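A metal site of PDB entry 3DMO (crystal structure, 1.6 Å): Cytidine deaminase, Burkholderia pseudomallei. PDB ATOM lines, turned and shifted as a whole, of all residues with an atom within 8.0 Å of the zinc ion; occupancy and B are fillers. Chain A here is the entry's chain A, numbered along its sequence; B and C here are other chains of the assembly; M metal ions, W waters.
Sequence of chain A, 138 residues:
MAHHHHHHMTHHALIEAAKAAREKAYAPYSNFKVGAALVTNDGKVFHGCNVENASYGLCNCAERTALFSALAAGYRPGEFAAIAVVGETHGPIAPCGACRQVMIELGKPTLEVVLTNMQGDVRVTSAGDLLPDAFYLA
Water W1 bridges OE2 of Glu 63 (2.7 Å) and N of Cys 96 (2.9 Å).
The zinc ion is bound by water W1 (2.1 Å), the side-chain sulfur of Cys 96 (2.2 Å), the side-chain sulfur of Cys 99 (2.4 Å) and the side-chain sulfur of Cys 61 (2.4 Å).
SG of Cys 96 lies close to N of Ala 98 (3.7 Å). OE1 of Glu 63 sits close to SG of Cys 99 (3.7 Å). NE of Arg 64 lies close to SG of Cys 99, at 3.5 Å. NH2 of Arg 64 sits close to SG of Cys 61 (3.3 Å). The side-chain sulfur of Cys 96 sits close to the side-chain hydroxyl of Ser 55 of chain B.
Within 4 Å of the zinc ion: Cys 61, Cys 96 and Cys 99. The nearest printed residue that does not touch the zinc ion is Glu 63 (4.03 Å).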
ATOM      1  N   VAL A  34     -14.842  -6.390  21.356  1.00  0.00           N
ATOM      2  CA  VAL A  34     -15.294  -7.744  21.652  1.00  0.00           C
ATOM      3  C   VAL A  34     -15.664  -7.813  23.133  1.00  0.00           C
ATOM      4  O   VAL A  34     -15.026  -7.174  23.971  1.00  0.00           O
ATOM      5  CB  VAL A  34     -14.210  -8.816  21.316  1.00  0.00           C
ATOM      6  CG1 VAL A  34     -14.751 -10.242  21.516  1.00  0.00           C
ATOM      7  CG2 VAL A  34     -13.699  -8.674  19.899  1.00  0.00           C
ATOM      8  N   ASN A  50     -11.778  -6.864  25.089  1.00  0.00           N
ATOM      9  CA  ASN A  50     -10.424  -6.703  24.570  1.00  0.00           C
ATOM     10  C   ASN A  50      -9.791  -5.415  25.089  1.00  0.00           C
ATOM     11  O   ASN A  50     -10.492  -4.422  25.351  1.00  0.00           O
ATOM     12  CB  ASN A  50     -10.342  -6.864  23.042  1.00  0.00           C
ATOM     13  CG  ASN A  50     -11.287  -5.938  22.285  1.00  0.00           C
ATOM     14  OD1 ASN A  50     -12.392  -5.651  22.737  1.00  0.00           O
ATOM     15  ND2 ASN A  50     -10.861  -5.524  21.094  1.00  0.00           N
ATOM     16  N   CYS A  59      -1.825  -6.585  23.051  1.00  0.00           N
ATOM     17  CA  CYS A  59      -3.290  -6.615  23.128  1.00  0.00           C
ATOM     18  C   CYS A  59      -3.755  -7.891  23.822  1.00  0.00           C
ATOM     19  O   CYS A  59      -3.147  -8.953  23.646  1.00  0.00           O
ATOM     20  CB  CYS A  59      -3.917  -6.544  21.731  1.00  0.00           C
ATOM     21  SG  CYS A  59      -3.618  -4.971  20.868  1.00  0.00           S
ATOM     22  N   ASN A  60      -4.815  -7.769  24.617  1.00  0.00           N
ATOM     23  CA  ASN A  60      -5.451  -8.932  25.229  1.00  0.00           C
ATOM     24  C   ASN A  60      -6.904  -9.053  24.777  1.00  0.00           C
ATOM     25  O   ASN A  60      -7.590  -8.047  24.652  1.00  0.00           O
ATOM     26  CB  ASN A  60      -5.389  -8.831  26.753  1.00  0.00           C
ATOM     27  CG  ASN A  60      -5.651 -10.169  27.433  1.00  0.00           C
ATOM     28  OD1 ASN A  60      -4.908 -11.138  27.219  1.00  0.00           O
ATOM     29  ND2 ASN A  60      -6.689 -10.234  28.257  1.00  0.00           N
ATOM     30  N   CYS A  61      -7.336 -10.290  24.560  1.00  0.00           N
ATOM     31  CA  CYS A  61      -8.685 -10.589  24.099  1.00  0.00           C
ATOM     32  C   CYS A  61      -9.697 -10.649  25.240  1.00  0.00           C
ATOM     33  O   CYS A  61      -9.333 -10.930  26.387  1.00  0.00           O
ATOM     34  CB  CYS A  61      -8.698 -11.934  23.390  1.00  0.00           C
ATOM     35  SG  CYS A  61      -7.799 -11.967  21.838  1.00  0.00           S
ATOM     36  N   ALA A  62     -10.972 -10.399  24.893  1.00  0.00           N
ATOM     37  CA  ALA A  62     -12.097 -10.481  25.829  1.00  0.00           C
ATOM     38  C   ALA A  62     -12.203 -11.782  26.622  1.00  0.00           C
ATOM     39  O   ALA A  62     -12.359 -11.760  27.841  1.00  0.00           O
ATOM     40  CB  ALA A  62     -13.413 -10.215  25.072  1.00  0.00           C
ATOM     41  N   GLU A  63     -12.086 -12.917  25.923  1.00  0.00           N
ATOM     42  CA  GLU A  63     -12.194 -14.234  26.539  1.00  0.00           C
ATOM     43  C   GLU A  63     -11.144 -14.371  27.645  1.00  0.00           C
ATOM     44  O   GLU A  63     -11.445 -14.805  28.763  1.00  0.00           O
ATOM     45  CB  GLU A  63     -11.962 -15.354  25.503  1.00  0.00           C
ATOM     46  CG  GLU A  63     -12.919 -15.368  24.300  1.00  0.00           C
ATOM     47  CD  GLU A  63     -12.416 -14.548  23.093  1.00  0.00           C
ATOM     48  OE1 GLU A  63     -12.093 -13.358  23.250  1.00  0.00           O
ATOM     49  OE2 GLU A  63     -12.349 -15.112  21.977  1.00  0.00           O
ATOM     50  N   ARG A  64      -9.911 -13.977  27.321  1.00  0.00           N
ATOM     51  CA  ARG A  64      -8.807 -14.072  28.270  1.00  0.00           C
ATOM     52  C   ARG A  64      -8.933 -13.092  29.429  1.00  0.00           C
ATOM     53  O   ARG A  64      -8.651 -13.455  30.566  1.00  0.00           O
ATOM     54  CB  ARG A  64      -7.457 -13.968  27.576  1.00  0.00           C
ATOM     55  CG  ARG A  64      -7.095 -15.247  26.822  1.00  0.00           C
ATOM     56  CD  ARG A  64      -5.750 -15.127  26.159  1.00  0.00           C
ATOM     57  NE  ARG A  64      -5.836 -14.376  24.911  1.00  0.00           N
ATOM     58  CZ  ARG A  64      -4.800 -13.836  24.274  1.00  0.00           C
ATOM     59  NH1 ARG A  64      -3.556 -13.956  24.765  1.00  0.00           N
ATOM     60  NH2 ARG A  64      -4.993 -13.173  23.146  1.00  0.00           N
ATOM     61  N   VAL A  85     -19.220 -15.208  23.973  1.00  0.00           N
ATOM     62  CA  VAL A  85     -18.321 -14.259  23.304  1.00  0.00           C
ATOM     63  C   VAL A  85     -19.119 -13.578  22.180  1.00  0.00           C
ATOM     64  O   VAL A  85     -19.855 -14.243  21.438  1.00  0.00           O
ATOM     65  CB  VAL A  85     -17.061 -14.961  22.714  1.00  0.00           C
ATOM     66  CG1 VAL A  85     -15.976 -13.936  22.325  1.00  0.00           C
ATOM     67  CG2 VAL A  85     -16.511 -15.988  23.688  1.00  0.00           C
ATOM     68  N   ALA A  94     -15.635 -16.033  16.066  1.00  0.00           N
ATOM     69  CA  ALA A  94     -14.726 -17.144  16.255  1.00  0.00           C
ATOM     70  C   ALA A  94     -13.597 -16.731  17.206  1.00  0.00           C
ATOM     71  O   ALA A  94     -12.863 -15.783  16.925  1.00  0.00           O
ATOM     72  CB  ALA A  94     -14.159 -17.546  14.933  1.00  0.00           C
ATOM     73  N   PRO A  95     -13.473 -17.417  18.354  1.00  0.00           N
ATOM     74  CA  PRO A  95     -12.323 -17.155  19.217  1.00  0.00           C
ATOM     75  C   PRO A  95     -11.003 -17.410  18.508  1.00  0.00           C
ATOM     76  O   PRO A  95     -10.882 -18.386  17.766  1.00  0.00           O
ATOM     77  CB  PRO A  95     -12.506 -18.172  20.355  1.00  0.00           C
ATOM     78  CG  PRO A  95     -13.997 -18.411  20.391  1.00  0.00           C
ATOM     79  CD  PRO A  95     -14.354 -18.447  18.936  1.00  0.00           C
ATOM     80  N   CYS A  96     -10.024 -16.540  18.755  1.00  0.00           N
ATOM     81  CA  CYS A  96      -8.693 -16.780  18.211  1.00  0.00           C
ATOM     82  C   CYS A  96      -8.033 -17.983  18.875  1.00  0.00           C
ATOM     83  O   CYS A  96      -8.457 -18.437  19.956  1.00  0.00           O
ATOM     84  CB  CYS A  96      -7.810 -15.528  18.336  1.00  0.00           C
ATOM     85  SG  CYS A  96      -7.047 -15.272  19.961  1.00  0.00           S
ATOM     86  N   GLY A  97      -6.986 -18.495  18.229  1.00  0.00           N
ATOM     87  CA  GLY A  97      -6.260 -19.678  18.702  1.00  0.00           C
ATOM     88  C   GLY A  97      -5.631 -19.533  20.085  1.00  0.00           C
ATOM     89  O   GLY A  97      -5.610 -20.491  20.878  1.00  0.00           O
ATOM     90  N   ALA A  98      -5.091 -18.355  20.376  1.00  0.00           N
ATOM     91  CA  ALA A  98      -4.557 -18.052  21.715  1.00  0.00           C
ATOM     92  C   ALA A  98      -5.644 -18.192  22.779  1.00  0.00           C
ATOM     93  O   ALA A  98      -5.444 -18.838  23.814  1.00  0.00           O
ATOM     94  CB  ALA A  98      -3.939 -16.670  21.741  1.00  0.00           C
ATOM     95  N   CYS A  99      -6.806 -17.571  22.534  1.00  0.00           N
ATOM     96  CA  CYS A  99      -7.942 -17.716  23.449  1.00  0.00           C
ATOM     97  C   CYS A  99      -8.422 -19.151  23.624  1.00  0.00           C
ATOM     98  O   CYS A  99      -8.785 -19.541  24.728  1.00  0.00           O
ATOM     99  CB  CYS A  99      -9.124 -16.847  23.005  1.00  0.00           C
ATOM    100  SG  CYS A  99      -8.881 -15.099  23.364  1.00  0.00           S
ATOM    101  N   ARG A 100      -8.409 -19.922  22.535  1.00  0.00           N
ATOM    102  CA  ARG A 100      -8.763 -21.350  22.582  1.00  0.00           C
ATOM    103  C   ARG A 100      -7.814 -22.147  23.483  1.00  0.00           C
ATOM    104  O   ARG A 100      -8.258 -23.020  24.227  1.00  0.00           O
ATOM    105  CB  ARG A 100      -8.829 -21.944  21.177  1.00  0.00           C
ATOM    106  CG  ARG A 100      -9.927 -21.352  20.312  1.00  0.00           C
ATOM    107  CD  ARG A 100      -9.939 -21.985  18.922  1.00  0.00           C
ATOM    108  NE  ARG A 100     -10.733 -21.194  17.978  1.00  0.00           N
ATOM    109  CZ  ARG A 100     -11.281 -21.654  16.851  1.00  0.00           C
ATOM    110  NH1 ARG A 100     -11.142 -22.929  16.485  1.00  0.00           N
ATOM    111  NH2 ARG A 100     -11.946 -20.822  16.077  1.00  0.00           N
ATOM    112  N   MET A 103      -8.664 -21.031  27.071  1.00  0.00           N
ATOM    113  CA  MET A 103      -9.949 -21.641  27.408  1.00  0.00           C
ATOM    114  C   MET A 103      -9.849 -23.117  27.713  1.00  0.00           C
ATOM    115  O   MET A 103     -10.498 -23.598  28.639  1.00  0.00           O
ATOM    116  CB  MET A 103     -10.984 -21.408  26.306  1.00  0.00           C
ATOM    117  CG  MET A 103     -11.516 -19.996  26.258  1.00  0.00           C
ATOM    118  SD  MET A 103     -12.931 -19.867  25.149  1.00  0.00           S
ATOM    119  CE  MET A 103     -12.168 -20.150  23.567  1.00  0.00           C
ATOM    120  N   ALA B  54      -4.217 -11.260  12.612  1.00  0.00           N
ATOM    121  CA  ALA B  54      -5.597 -10.821  12.885  1.00  0.00           C
ATOM    122  C   ALA B  54      -5.896 -10.786  14.377  1.00  0.00           C
ATOM    123  O   ALA B  54      -6.657  -9.926  14.850  1.00  0.00           O
ATOM    124  CB  ALA B  54      -6.576 -11.734  12.167  1.00  0.00           C
ATOM    125  N   SER B  55      -5.327 -11.734  15.123  1.00  0.00           N
ATOM    126  CA  SER B  55      -5.323 -11.687  16.573  1.00  0.00           C
ATOM    127  C   SER B  55      -4.120 -10.831  16.977  1.00  0.00           C
ATOM    128  O   SER B  55      -2.975 -11.291  16.945  1.00  0.00           O
ATOM    129  CB  SER B  55      -5.201 -13.089  17.153  1.00  0.00           C
ATOM    130  OG  SER B  55      -5.274 -13.032  18.572  1.00  0.00           O
ATOM    131  N   TYR B  56      -4.380  -9.584  17.370  1.00  0.00           N
ATOM    132  CA  TYR B  56      -3.292  -8.608  17.540  1.00  0.00           C
ATOM    133  C   TYR B  56      -2.202  -9.054  18.512  1.00  0.00           C
ATOM    134  O   TYR B  56      -1.039  -8.790  18.277  1.00  0.00           O
ATOM    135  CB  TYR B  56      -3.843  -7.228  17.948  1.00  0.00           C
ATOM    136  CG  TYR B  56      -4.411  -6.381  16.814  1.00  0.00           C
ATOM    137  CD1 TYR B  56      -4.616  -5.012  17.001  1.00  0.00           C
ATOM    138  CD2 TYR B  56      -4.726  -6.938  15.565  1.00  0.00           C
ATOM    139  CE1 TYR B  56      -5.146  -4.213  15.977  1.00  0.00           C
ATOM    140  CE2 TYR B  56      -5.247  -6.145  14.540  1.00  0.00           C
ATOM    141  CZ  TYR B  56      -5.454  -4.790  14.753  1.00  0.00           C
ATOM    142  OH  TYR B  56      -5.968  -4.012  13.743  1.00  0.00           O
ATOM    143  N   GLY B  57      -2.587  -9.746  19.586  1.00  0.00           N
ATOM    144  CA  GLY B  57      -1.645 -10.196  20.607  1.00  0.00           C
ATOM    145  C   GLY B  57      -0.619 -11.161  20.055  1.00  0.00           C
ATOM    146  O   GLY B  57       0.413 -11.407  20.690  1.00  0.00           O
ATOM    147  N   LEU B  58      -0.886 -11.692  18.867  1.00  0.00           N
ATOM    148  CA  LEU B  58       0.078 -12.618  18.232  1.00  0.00           C
ATOM    149  C   LEU B  58       1.034 -11.936  17.271  1.00  0.00           C
ATOM    150  O   LEU B  58       1.912 -12.591  16.704  1.00  0.00           O
ATOM    151  CB  LEU B  58      -0.639 -13.815  17.567  1.00  0.00           C
ATOM    152  CG  LEU B  58      -1.439 -14.668  18.557  1.00  0.00           C
ATOM    153  CD1 LEU B  58      -2.319 -15.684  17.856  1.00  0.00           C
ATOM    154  CD2 LEU B  58      -0.506 -15.324  19.586  1.00  0.00           C
ATOM    155  N   GLN C 101      -3.021 -20.243  15.083  1.00  0.00           N
ATOM    156  CA  GLN C 101      -3.549 -18.975  14.591  1.00  0.00           C
ATOM    157  C   GLN C 101      -2.591 -18.297  13.606  1.00  0.00           C
ATOM    158  O   GLN C 101      -3.009 -17.744  12.584  1.00  0.00           O
ATOM    159  CB  GLN C 101      -3.864 -18.044  15.765  1.00  0.00           C
ATOM    160  CG  GLN C 101      -4.645 -16.782  15.386  1.00  0.00           C
ATOM    161  CD  GLN C 101      -6.044 -17.086  14.853  1.00  0.00           C
ATOM    162  OE1 GLN C 101      -6.844 -17.748  15.514  1.00  0.00           O
ATOM    163  NE2 GLN C 101      -6.326 -16.612  13.638  1.00  0.00           N
ATOM    164  N   PHE C 135     -10.650 -17.631  13.430  1.00  0.00           N
ATOM    165  CA  PHE C 135     -10.837 -16.183  13.467  1.00  0.00           C
ATOM    166  C   PHE C 135     -10.031 -15.512  12.362  1.00  0.00           C
ATOM    167  O   PHE C 135      -8.861 -15.818  12.162  1.00  0.00           O
ATOM    168  CB  PHE C 135     -10.419 -15.619  14.834  1.00  0.00           C
ATOM    169  CG  PHE C 135     -10.482 -14.119  14.924  1.00  0.00           C
ATOM    170  CD1 PHE C 135     -11.705 -13.466  15.053  1.00  0.00           C
ATOM    171  CD2 PHE C 135      -9.312 -13.357  14.897  1.00  0.00           C
ATOM    172  CE1 PHE C 135     -11.762 -12.066  15.136  1.00  0.00           C
ATOM    173  CE2 PHE C 135      -9.366 -11.969  14.975  1.00  0.00           C
ATOM    174  CZ  PHE C 135     -10.589 -11.316  15.104  1.00  0.00           C
HETATM  175 ZN    ZN M   1      -8.501 -14.174  21.208  1.00  0.00          ZN
HETATM  176  O   HOH W   1     -10.436 -14.109  20.309  1.00  0.00           O
